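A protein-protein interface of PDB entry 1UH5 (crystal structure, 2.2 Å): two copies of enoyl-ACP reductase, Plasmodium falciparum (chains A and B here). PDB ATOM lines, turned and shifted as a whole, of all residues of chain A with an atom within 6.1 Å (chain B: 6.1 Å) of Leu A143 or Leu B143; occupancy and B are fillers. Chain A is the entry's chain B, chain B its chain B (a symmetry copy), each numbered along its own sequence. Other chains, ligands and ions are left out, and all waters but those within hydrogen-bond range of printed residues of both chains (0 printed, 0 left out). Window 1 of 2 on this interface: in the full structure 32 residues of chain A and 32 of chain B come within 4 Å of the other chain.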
ATOM      1  N   ASN A 123       6.112  -5.980 -14.072  1.00  0.00           N
ATOM      2  CA  ASN A 123       6.325  -6.858 -15.206  1.00  0.00           C
ATOM      3  C   ASN A 123       7.490  -6.341 -16.029  1.00  0.00           C
ATOM      4  O   ASN A 123       7.696  -5.132 -16.142  1.00  0.00           O
ATOM      5  CB  ASN A 123       5.059  -6.930 -16.063  1.00  0.00           C
ATOM      6  CG  ASN A 123       4.812  -8.321 -16.621  1.00  0.00           C
ATOM      7  OD1 ASN A 123       3.749  -8.596 -17.179  1.00  0.00           O
ATOM      8  ND2 ASN A 123       5.795  -9.206 -16.475  1.00  0.00           N
ATOM      9  N   ARG A 136      16.647  -1.795 -25.323  1.00  0.00           N
ATOM     10  CA  ARG A 136      15.916  -0.562 -25.046  1.00  0.00           C
ATOM     11  C   ARG A 136      14.437  -0.893 -24.854  1.00  0.00           C
ATOM     12  O   ARG A 136      13.805  -0.426 -23.902  1.00  0.00           O
ATOM     13  CB  ARG A 136      16.095   0.442 -26.196  1.00  0.00           C
ATOM     14  CG  ARG A 136      15.529   1.835 -25.908  1.00  0.00           C
ATOM     15  CD  ARG A 136      15.846   2.820 -27.037  1.00  0.00           C
ATOM     16  NE  ARG A 136      17.284   3.028 -27.215  1.00  0.00           N
ATOM     17  CZ  ARG A 136      17.953   4.102 -26.804  1.00  0.00           C
ATOM     18  NH1 ARG A 136      17.322   5.090 -26.182  1.00  0.00           N
ATOM     19  NH2 ARG A 136      19.258   4.192 -27.019  1.00  0.00           N
ATOM     20  N   GLY A 138      13.019  -3.749 -23.930  1.00  0.00           N
ATOM     21  CA  GLY A 138      12.781  -4.456 -22.681  1.00  0.00           C
ATOM     22  C   GLY A 138      12.797  -3.514 -21.484  1.00  0.00           C
ATOM     23  O   GLY A 138      11.964  -3.614 -20.585  1.00  0.00           O
ATOM     24  N   TYR A 139      13.753  -2.592 -21.490  1.00  0.00           N
ATOM     25  CA  TYR A 139      13.912  -1.607 -20.426  1.00  0.00           C
ATOM     26  C   TYR A 139      12.665  -0.733 -20.297  1.00  0.00           C
ATOM     27  O   TYR A 139      12.092  -0.604 -19.212  1.00  0.00           O
ATOM     28  CB  TYR A 139      15.137  -0.743 -20.733  1.00  0.00           C
ATOM     29  CG  TYR A 139      15.550   0.230 -19.649  1.00  0.00           C
ATOM     30  CD1 TYR A 139      15.165   1.567 -19.702  1.00  0.00           C
ATOM     31  CD2 TYR A 139      16.386  -0.178 -18.607  1.00  0.00           C
ATOM     32  CE1 TYR A 139      15.611   2.483 -18.751  1.00  0.00           C
ATOM     33  CE2 TYR A 139      16.837   0.723 -17.649  1.00  0.00           C
ATOM     34  CZ  TYR A 139      16.450   2.052 -17.730  1.00  0.00           C
ATOM     35  OH  TYR A 139      16.928   2.951 -16.812  1.00  0.00           O
ATOM     36  N   LEU A 140      12.247  -0.137 -21.410  1.00  0.00           N
ATOM     37  CA  LEU A 140      11.074   0.727 -21.416  1.00  0.00           C
ATOM     38  C   LEU A 140       9.818  -0.059 -21.061  1.00  0.00           C
ATOM     39  O   LEU A 140       8.902   0.476 -20.442  1.00  0.00           O
ATOM     40  CB  LEU A 140      10.913   1.406 -22.782  1.00  0.00           C
ATOM     41  CG  LEU A 140      12.035   2.373 -23.172  1.00  0.00           C
ATOM     42  CD1 LEU A 140      11.704   3.004 -24.525  1.00  0.00           C
ATOM     43  CD2 LEU A 140      12.203   3.457 -22.101  1.00  0.00           C
ATOM     44  N   ASP A 141       9.774  -1.330 -21.448  1.00  0.00           N
ATOM     45  CA  ASP A 141       8.627  -2.165 -21.109  1.00  0.00           C
ATOM     46  C   ASP A 141       8.532  -2.291 -19.583  1.00  0.00           C
ATOM     47  O   ASP A 141       7.449  -2.210 -19.006  1.00  0.00           O
ATOM     48  CB  ASP A 141       8.773  -3.555 -21.742  1.00  0.00           C
ATOM     49  CG  ASP A 141       7.686  -4.518 -21.293  1.00  0.00           C
ATOM     50  OD1 ASP A 141       7.950  -5.355 -20.397  1.00  0.00           O
ATOM     51  OD2 ASP A 141       6.563  -4.427 -21.827  1.00  0.00           O
ATOM     52  N   ALA A 142       9.674  -2.484 -18.930  1.00  0.00           N
ATOM     53  CA  ALA A 142       9.701  -2.614 -17.474  1.00  0.00           C
ATOM     54  C   ALA A 142       9.226  -1.318 -16.807  1.00  0.00           C
ATOM     55  O   ALA A 142       8.387  -1.343 -15.908  1.00  0.00           O
ATOM     56  CB  ALA A 142      11.119  -2.966 -17.002  1.00  0.00           C
ATOM     57  N   LEU A 143       9.753  -0.186 -17.263  1.00  0.00           N
ATOM     58  CA  LEU A 143       9.371   1.112 -16.703  1.00  0.00           C
ATOM     59  C   LEU A 143       7.905   1.443 -16.955  1.00  0.00           C
ATOM     60  O   LEU A 143       7.216   1.960 -16.078  1.00  0.00           O
ATOM     61  CB  LEU A 143      10.244   2.228 -17.295  1.00  0.00           C
ATOM     62  CG  LEU A 143      11.571   2.558 -16.604  1.00  0.00           C
ATOM     63  CD1 LEU A 143      11.302   3.148 -15.224  1.00  0.00           C
ATOM     64  CD2 LEU A 143      12.427   1.314 -16.496  1.00  0.00           C
ATOM     65  N   SER A 144       7.435   1.144 -18.161  1.00  0.00           N
ATOM     66  CA  SER A 144       6.057   1.425 -18.540  1.00  0.00           C
ATOM     67  C   SER A 144       5.048   0.723 -17.638  1.00  0.00           C
ATOM     68  O   SER A 144       4.166   1.353 -17.053  1.00  0.00           O
ATOM     69  CB  SER A 144       5.808   0.996 -19.993  1.00  0.00           C
ATOM     70  OG  SER A 144       4.488   1.321 -20.395  1.00  0.00           O
ATOM     71  N   LYS A 145       5.195  -0.588 -17.526  1.00  0.00           N
ATOM     72  CA  LYS A 145       4.280  -1.393 -16.736  1.00  0.00           C
ATOM     73  C   LYS A 145       4.503  -1.387 -15.233  1.00  0.00           C
ATOM     74  O   LYS A 145       3.539  -1.427 -14.467  1.00  0.00           O
ATOM     75  CB  LYS A 145       4.309  -2.827 -17.268  1.00  0.00           C
ATOM     76  CG  LYS A 145       3.906  -2.883 -18.728  1.00  0.00           C
ATOM     77  CD  LYS A 145       4.093  -4.248 -19.333  1.00  0.00           C
ATOM     78  CE  LYS A 145       3.677  -4.214 -20.810  1.00  0.00           C
ATOM     79  NZ  LYS A 145       4.077  -5.480 -21.483  1.00  0.00           N
ATOM     80  N   SER A 146       5.761  -1.320 -14.808  1.00  0.00           N
ATOM     81  CA  SER A 146       6.081  -1.352 -13.382  1.00  0.00           C
ATOM     82  C   SER A 146       6.128  -0.003 -12.666  1.00  0.00           C
ATOM     83  O   SER A 146       5.874   0.065 -11.464  1.00  0.00           O
ATOM     84  CB  SER A 146       7.420  -2.069 -13.161  1.00  0.00           C
ATOM     85  OG  SER A 146       7.415  -3.359 -13.751  1.00  0.00           O
ATOM     86  N   SER A 147       6.449   1.063 -13.394  1.00  0.00           N
ATOM     87  CA  SER A 147       6.556   2.379 -12.775  1.00  0.00           C
ATOM     88  C   SER A 147       5.521   3.397 -13.248  1.00  0.00           C
ATOM     89  O   SER A 147       4.789   3.961 -12.432  1.00  0.00           O
ATOM     90  CB  SER A 147       7.959   2.938 -13.006  1.00  0.00           C
ATOM     91  OG  SER A 147       8.938   1.973 -12.670  1.00  0.00           O
ATOM     92  N   TYR A 148       5.455   3.636 -14.555  1.00  0.00           N
ATOM     93  CA  TYR A 148       4.504   4.619 -15.057  1.00  0.00           C
ATOM     94  C   TYR A 148       3.081   4.274 -14.660  1.00  0.00           C
ATOM     95  O   TYR A 148       2.264   5.165 -14.429  1.00  0.00           O
ATOM     96  CB  TYR A 148       4.559   4.758 -16.584  1.00  0.00           C
ATOM     97  CG  TYR A 148       3.660   5.888 -17.046  1.00  0.00           C
ATOM     98  CD1 TYR A 148       4.046   7.216 -16.867  1.00  0.00           C
ATOM     99  CD2 TYR A 148       2.369   5.637 -17.522  1.00  0.00           C
ATOM    100  CE1 TYR A 148       3.171   8.270 -17.130  1.00  0.00           C
ATOM    101  CE2 TYR A 148       1.476   6.692 -17.789  1.00  0.00           C
ATOM    102  CZ  TYR A 148       1.889   8.005 -17.584  1.00  0.00           C
ATOM    103  OH  TYR A 148       1.024   9.058 -17.798  1.00  0.00           O
ATOM    104  N   SER A 149       2.786   2.981 -14.590  1.00  0.00           N
ATOM    105  CA  SER A 149       1.451   2.533 -14.231  1.00  0.00           C
ATOM    106  C   SER A 149       0.972   3.157 -12.922  1.00  0.00           C
ATOM    107  O   SER A 149      -0.215   3.431 -12.764  1.00  0.00           O
ATOM    108  CB  SER A 149       1.415   1.002 -14.132  1.00  0.00           C
ATOM    109  OG  SER A 149       2.406   0.510 -13.244  1.00  0.00           O
ATOM    110  N   GLY A 185      15.774  -4.450 -16.071  1.00  0.00           N
ATOM    111  CA  GLY A 185      15.444  -3.074 -15.759  1.00  0.00           C
ATOM    112  C   GLY A 185      14.477  -2.982 -14.588  1.00  0.00           C
ATOM    113  O   GLY A 185      13.969  -1.905 -14.286  1.00  0.00           O
ATOM    114  N   SER A 188      15.776  -0.694 -12.111  1.00  0.00           N
ATOM    115  CA  SER A 188      15.608   0.666 -12.610  1.00  0.00           C
ATOM    116  C   SER A 188      14.178   1.121 -12.342  1.00  0.00           C
ATOM    117  O   SER A 188      13.941   2.228 -11.861  1.00  0.00           O
ATOM    118  CB  SER A 188      15.885   0.706 -14.117  1.00  0.00           C
ATOM    119  OG  SER A 188      17.025  -0.072 -14.447  1.00  0.00           O
ATOM    120  N   ALA A 189      13.229   0.250 -12.657  1.00  0.00           N
ATOM    121  CA  ALA A 189      11.817   0.540 -12.464  1.00  0.00           C
ATOM    122  C   ALA A 189      11.478   0.808 -10.992  1.00  0.00           C
ATOM    123  O   ALA A 189      10.700   1.709 -10.687  1.00  0.00           O
ATOM    124  CB  ALA A 189      10.981  -0.615 -12.994  1.00  0.00           C
ATOM    125  N   LYS A 190      12.053   0.017 -10.089  1.00  0.00           N
ATOM    126  CA  LYS A 190      11.802   0.195  -8.660  1.00  0.00           C
ATOM    127  C   LYS A 190      12.426   1.495  -8.128  1.00  0.00           C
ATOM    128  O   LYS A 190      11.861   2.147  -7.254  1.00  0.00           O
ATOM    129  CB  LYS A 190      12.330  -1.010  -7.882  1.00  0.00           C
ATOM    130  CG  LYS A 190      11.556  -2.298  -8.163  1.00  0.00           C
ATOM    131  CD  LYS A 190      10.062  -2.135  -7.878  1.00  0.00           C
ATOM    132  CE  LYS A 190       9.336  -3.462  -8.002  1.00  0.00           C
ATOM    133  NZ  LYS A 190       7.877  -3.328  -7.783  1.00  0.00           N
ATOM    134  N   ALA A 192      12.793   4.190  -9.859  1.00  0.00           N
ATOM    135  CA  ALA A 192      11.922   5.235 -10.387  1.00  0.00           C
ATOM    136  C   ALA A 192      10.637   5.286  -9.551  1.00  0.00           C
ATOM    137  O   ALA A 192      10.146   6.363  -9.205  1.00  0.00           O
ATOM    138  CB  ALA A 192      11.588   4.950 -11.866  1.00  0.00           C
ATOM    139  N   ASN B 123      17.207  14.483 -21.947  1.00  0.00           N
ATOM    140  CA  ASN B 123      16.159  15.065 -22.763  1.00  0.00           C
ATOM    141  C   ASN B 123      14.820  14.486 -22.346  1.00  0.00           C
ATOM    142  O   ASN B 123      14.727  13.317 -21.968  1.00  0.00           O
ATOM    143  CB  ASN B 123      16.423  14.780 -24.243  1.00  0.00           C
ATOM    144  CG  ASN B 123      16.048  15.949 -25.137  1.00  0.00           C
ATOM    145  OD1 ASN B 123      16.362  15.958 -26.327  1.00  0.00           O
ATOM    146  ND2 ASN B 123      15.372  16.944 -24.566  1.00  0.00           N
ATOM    147  N   ARG B 136       2.342   8.758 -20.803  1.00  0.00           N
ATOM    148  CA  ARG B 136       3.180   7.563 -20.827  1.00  0.00           C
ATOM    149  C   ARG B 136       4.310   7.769 -21.835  1.00  0.00           C
ATOM    150  O   ARG B 136       5.476   7.492 -21.541  1.00  0.00           O
ATOM    151  CB  ARG B 136       2.348   6.327 -21.202  1.00  0.00           C
ATOM    152  CG  ARG B 136       3.097   4.998 -21.063  1.00  0.00           C
ATOM    153  CD  ARG B 136       2.182   3.800 -21.331  1.00  0.00           C
ATOM    154  NE  ARG B 136       1.077   3.712 -20.374  1.00  0.00           N
ATOM    155  CZ  ARG B 136       1.020   2.855 -19.358  1.00  0.00           C
ATOM    156  NH1 ARG B 136       2.009   1.994 -19.147  1.00  0.00           N
ATOM    157  NH2 ARG B 136      -0.031   2.855 -18.549  1.00  0.00           N
ATOM    158  N   GLY B 138       5.643  10.595 -22.957  1.00  0.00           N
ATOM    159  CA  GLY B 138       6.620  11.565 -22.484  1.00  0.00           C
ATOM    160  C   GLY B 138       7.560  10.963 -21.448  1.00  0.00           C
ATOM    161  O   GLY B 138       8.767  11.196 -21.473  1.00  0.00           O
ATOM    162  N   TYR B 139       6.991  10.179 -20.540  1.00  0.00           N
ATOM    163  CA  TYR B 139       7.742   9.518 -19.478  1.00  0.00           C
ATOM    164  C   TYR B 139       8.796   8.575 -20.059  1.00  0.00           C
ATOM    165  O   TYR B 139       9.979   8.663 -19.719  1.00  0.00           O
ATOM    166  CB  TYR B 139       6.766   8.743 -18.592  1.00  0.00           C
ATOM    167  CG  TYR B 139       7.354   8.126 -17.341  1.00  0.00           C
ATOM    168  CD1 TYR B 139       7.728   6.785 -17.311  1.00  0.00           C
ATOM    169  CD2 TYR B 139       7.468   8.872 -16.166  1.00  0.00           C
ATOM    170  CE1 TYR B 139       8.192   6.193 -16.138  1.00  0.00           C
ATOM    171  CE2 TYR B 139       7.931   8.297 -14.988  1.00  0.00           C
ATOM    172  CZ  TYR B 139       8.288   6.956 -14.980  1.00  0.00           C
ATOM    173  OH  TYR B 139       8.704   6.375 -13.810  1.00  0.00           O
ATOM    174  N   LEU B 140       8.362   7.676 -20.936  1.00  0.00           N
ATOM    175  CA  LEU B 140       9.268   6.717 -21.555  1.00  0.00           C
ATOM    176  C   LEU B 140      10.307   7.426 -22.412  1.00  0.00           C
ATOM    177  O   LEU B 140      11.442   6.969 -22.521  1.00  0.00           O
ATOM    178  CB  LEU B 140       8.482   5.701 -22.395  1.00  0.00           C
ATOM    179  CG  LEU B 140       7.529   4.795 -21.610  1.00  0.00           C
ATOM    180  CD1 LEU B 140       6.867   3.810 -22.575  1.00  0.00           C
ATOM    181  CD2 LEU B 140       8.291   4.041 -20.514  1.00  0.00           C
ATOM    182  N   ASP B 141       9.926   8.545 -23.019  1.00  0.00           N
ATOM    183  CA  ASP B 141      10.874   9.310 -23.821  1.00  0.00           C
ATOM    184  C   ASP B 141      12.010   9.806 -22.918  1.00  0.00           C
ATOM    185  O   ASP B 141      13.182   9.757 -23.287  1.00  0.00           O
ATOM    186  CB  ASP B 141      10.172  10.502 -24.485  1.00  0.00           C
ATOM    187  CG  ASP B 141      11.143  11.424 -25.205  1.00  0.00           C
ATOM    188  OD1 ASP B 141      11.505  12.484 -24.641  1.00  0.00           O
ATOM    189  OD2 ASP B 141      11.555  11.080 -26.331  1.00  0.00           O
ATOM    190  N   ALA B 142      11.658  10.280 -21.727  1.00  0.00           N
ATOM    191  CA  ALA B 142      12.659  10.776 -20.783  1.00  0.00           C
ATOM    192  C   ALA B 142      13.603   9.647 -20.355  1.00  0.00           C
ATOM    193  O   ALA B 142      14.823   9.808 -20.367  1.00  0.00           O
ATOM    194  CB  ALA B 142      11.971  11.388 -19.556  1.00  0.00           C
ATOM    195  N   LEU B 143      13.036   8.501 -19.994  1.00  0.00           N
ATOM    196  CA  LEU B 143      13.840   7.353 -19.570  1.00  0.00           C
ATOM    197  C   LEU B 143      14.717   6.812 -20.693  1.00  0.00           C
ATOM    198  O   LEU B 143      15.875   6.462 -20.474  1.00  0.00           O
ATOM    199  CB  LEU B 143      12.934   6.224 -19.057  1.00  0.00           C
ATOM    200  CG  LEU B 143      12.536   6.226 -17.577  1.00  0.00           C
ATOM    201  CD1 LEU B 143      13.767   5.978 -16.713  1.00  0.00           C
ATOM    202  CD2 LEU B 143      11.882   7.542 -17.212  1.00  0.00           C
ATOM    203  N   SER B 144      14.155   6.744 -21.894  1.00  0.00           N
ATOM    204  CA  SER B 144      14.875   6.229 -23.051  1.00  0.00           C
ATOM    205  C   SER B 144      16.141   7.023 -23.352  1.00  0.00           C
ATOM    206  O   SER B 144      17.238   6.469 -23.435  1.00  0.00           O
ATOM    207  CB  SER B 144      13.970   6.247 -24.291  1.00  0.00           C
ATOM    208  OG  SER B 144      14.638   5.690 -25.411  1.00  0.00           O
ATOM    209  N   LYS B 145      15.976   8.327 -23.506  1.00  0.00           N
ATOM    210  CA  LYS B 145      17.087   9.202 -23.840  1.00  0.00           C
ATOM    211  C   LYS B 145      18.000   9.600 -22.692  1.00  0.00           C
ATOM    212  O   LYS B 145      19.210   9.728 -22.883  1.00  0.00           O
ATOM    213  CB  LYS B 145      16.534  10.449 -24.530  1.00  0.00           C
ATOM    214  CG  LYS B 145      15.771  10.090 -25.790  1.00  0.00           C
ATOM    215  CD  LYS B 145      15.064  11.270 -26.400  1.00  0.00           C
ATOM    216  CE  LYS B 145      14.308  10.819 -27.657  1.00  0.00           C
ATOM    217  NZ  LYS B 145      13.414  11.910 -28.136  1.00  0.00           N
ATOM    218  N   SER B 146      17.434   9.779 -21.502  1.00  0.00           N
ATOM    219  CA  SER B 146      18.221  10.205 -20.346  1.00  0.00           C
ATOM    220  C   SER B 146      18.842   9.094 -19.501  1.00  0.00           C
ATOM    221  O   SER B 146      19.880   9.305 -18.875  1.00  0.00           O
ATOM    222  CB  SER B 146      17.368  11.095 -19.431  1.00  0.00           C
ATOM    223  OG  SER B 146      16.813  12.186 -20.148  1.00  0.00           O
ATOM    224  N   SER B 147      18.217   7.920 -19.482  1.00  0.00           N
ATOM    225  CA  SER B 147      18.724   6.822 -18.667  1.00  0.00           C
ATOM    226  C   SER B 147      19.219   5.612 -19.455  1.00  0.00           C
ATOM    227  O   SER B 147      20.369   5.197 -19.297  1.00  0.00           O
ATOM    228  CB  SER B 147      17.645   6.378 -17.682  1.00  0.00           C
ATOM    229  OG  SER B 147      17.098   7.497 -17.009  1.00  0.00           O
ATOM    230  N   TYR B 148      18.362   5.045 -20.301  1.00  0.00           N
ATOM    231  CA  TYR B 148      18.774   3.870 -21.058  1.00  0.00           C
ATOM    232  C   TYR B 148      20.009   4.148 -21.895  1.00  0.00           C
ATOM    233  O   TYR B 148      20.838   3.262 -22.098  1.00  0.00           O
ATOM    234  CB  TYR B 148      17.667   3.357 -21.988  1.00  0.00           C
ATOM    235  CG  TYR B 148      18.086   2.056 -22.644  1.00  0.00           C
ATOM    236  CD1 TYR B 148      18.089   0.866 -21.916  1.00  0.00           C
ATOM    237  CD2 TYR B 148      18.619   2.037 -23.937  1.00  0.00           C
ATOM    238  CE1 TYR B 148      18.625  -0.308 -22.444  1.00  0.00           C
ATOM    239  CE2 TYR B 148      19.165   0.859 -24.480  1.00  0.00           C
ATOM    240  CZ  TYR B 148      19.166  -0.307 -23.720  1.00  0.00           C
ATOM    241  OH  TYR B 148      19.729  -1.468 -24.208  1.00  0.00           O
ATOM    242  N   SER B 149      20.124   5.377 -22.385  1.00  0.00           N
ATOM    243  CA  SER B 149      21.259   5.754 -23.210  1.00  0.00           C
ATOM    244  C   SER B 149      22.590   5.433 -22.533  1.00  0.00           C
ATOM    245  O   SER B 149      23.557   5.080 -23.202  1.00  0.00           O
ATOM    246  CB  SER B 149      21.189   7.247 -23.558  1.00  0.00           C
ATOM    247  OG  SER B 149      21.077   8.051 -22.394  1.00  0.00           O
ATOM    248  N   GLY B 185       9.232  13.554 -16.013  1.00  0.00           N
ATOM    249  CA  GLY B 185       9.832  12.274 -15.694  1.00  0.00           C
ATOM    250  C   GLY B 185      11.346  12.377 -15.588  1.00  0.00           C
ATOM    251  O   GLY B 185      12.030  11.363 -15.478  1.00  0.00           O
ATOM    252  N   SER B 188      12.449  10.943 -12.460  1.00  0.00           N
ATOM    253  CA  SER B 188      12.359   9.491 -12.563  1.00  0.00           C
ATOM    254  C   SER B 188      13.593   8.966 -13.288  1.00  0.00           C
ATOM    255  O   SER B 188      14.220   7.998 -12.860  1.00  0.00           O
ATOM    256  CB  SER B 188      11.100   9.102 -13.347  1.00  0.00           C
ATOM    257  OG  SER B 188       9.988   9.890 -12.951  1.00  0.00           O
ATOM    258  N   ALA B 189      13.936   9.622 -14.389  1.00  0.00           N
ATOM    259  CA  ALA B 189      15.087   9.238 -15.191  1.00  0.00           C
ATOM    260  C   ALA B 189      16.396   9.317 -14.397  1.00  0.00           C
ATOM    261  O   ALA B 189      17.252   8.443 -14.521  1.00  0.00           O
ATOM    262  CB  ALA B 189      15.167  10.125 -16.425  1.00  0.00           C
ATOM    263  N   LYS B 190      16.553  10.367 -13.595  1.00  0.00           N
ATOM    264  CA  LYS B 190      17.762  10.530 -12.790  1.00  0.00           C
ATOM    265  C   LYS B 190      17.845   9.483 -11.668  1.00  0.00           C
ATOM    266  O   LYS B 190      18.931   9.015 -11.330  1.00  0.00           O
ATOM    267  CB  LYS B 190      17.816  11.942 -12.208  1.00  0.00           C
ATOM    268  CG  LYS B 190      18.015  13.026 -13.267  1.00  0.00           C
ATOM    269  CD  LYS B 190      19.275  12.780 -14.099  1.00  0.00           C
ATOM    270  CE  LYS B 190      19.548  13.946 -15.032  1.00  0.00           C
ATOM    271  NZ  LYS B 190      20.733  13.714 -15.890  1.00  0.00           N
ATOM    272  N   ALA B 192      16.654   6.493 -11.865  1.00  0.00           N
ATOM    273  CA  ALA B 192      16.997   5.261 -12.565  1.00  0.00           C
ATOM    274  C   ALA B 192      18.490   5.284 -12.915  1.00  0.00           C
ATOM    275  O   ALA B 192      19.194   4.283 -12.765  1.00  0.00           O
ATOM    276  CB  ALA B 192      16.148   5.125 -13.847  1.00  0.00           C
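The side-chain hydroxyl (OG) of Ser B144 lies within hydrogen-bond range of the guanidinium group (NH1) of Arg A136 (2.9 Å). N of Arg A136 is in hydrogen-bond range of OH of Tyr B148 (3.3 Å). The guanidinium group of Arg B136 lies within hydrogen-bond range of the side-chain hydroxyl of Ser A144, at 2.9 Å. OH of Tyr A148 is in hydrogen-bond range of N of Arg B136, at 3.3 Å.
The backbone carbonyl oxygen of Leu A143 sits at hydrogen-bond distance from the backbone NH of Tyr A148 (2.9 Å). The backbone carbonyl oxygen (O) of Ser A144 sits at hydrogen-bond distance from the backbone NH (N) of Ser A149 (3.3 Å). OG of Ser A147 is in hydrogen-bond range of O of Ala A189 (2.7 Å). O of Leu B143 lies within hydrogen-bond range of N of Tyr B148, at 2.9 Å. The backbone NH (N) of Ser B149 lies within hydrogen-bond range of the backbone carbonyl oxygen (O) of Ser B144, 3.3 Å away. OG of Ser B147 lies within hydrogen-bond range of O of Ala B189 (2.7 Å).
Ser B147 touches Tyr A139 (CB to OH, 3.6 Å). Tyr A139 touches Tyr B148 (CG to CD1, 3.5 Å). CB of Ala B192 touches OH of Tyr A139, 3.8 Å away. Leu A140 touches Leu B140. Leu A140 touches Ser B144. Leu A143 touches Leu B143 (CG to CG, 3.9 Å). Leu B140 touches Ser A144 (CD2 to N, 3.8 Å). OH of Tyr B139 touches CB of Ser A147, 3.6 Å away. Tyr A148 touches Tyr B139. CB of Ala A192 touches OH of Tyr B139 (3.8 Å).
Of the printed residues of chain B, Tyr A139 touches Ser B147 (3.6 Å), Tyr B148 (3.5 Å) and Ala B192 (3.8 Å). Of the printed residues of chain B, Ser A144 touches Arg B136 (2.9 Å) and Leu B140 (3.8 Å). Ser A149 touches none of the printed residues of chain B. Asn B123 touches none of the printed residues of chain A. Of the printed residues of chain A, Arg B136 touches Ser A144 (2.9 Å) and Tyr A148 (3.3 Å). Of the printed residues of chain A, Tyr B139 touches Ser A147 (3.6 Å), Tyr A148 (3.5 Å) and Ala A192 (3.8 Å). Leu B143 touches one residue of chain A. Printed residues of chain A within 4 Å of Ser B147: Tyr A139 (3.6 Å). The nearest residue of chain B that does not touch Leu A143 is Leu B140 (4.2 Å).
Of the 19 printed residues of chain B, 8 touch a printed residue of chain A. Hydrophobic or aromatic side chains of chain B within 4 Å of the printed part of chain A: Tyr B139, Leu B140, Leu B143, Tyr B148 and Ala B192. Hydrophobic or aromatic side chains of chain A that line the printed part of chain B: Tyr A139, Leu A140, Leu A143, Tyr A148 and Ala A192.
Arg A136 touches Tyr B148, and with the chains exchanged Tyr A148 touches Arg B136. Tyr A139 touches Ser B147, and with the chains exchanged Ser A147 touches Tyr B139. Leu A140 touches Ser B144, and with the chains exchanged Ser A144 touches Leu B140. Leu A143 touches its own counterpart, Leu B143.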
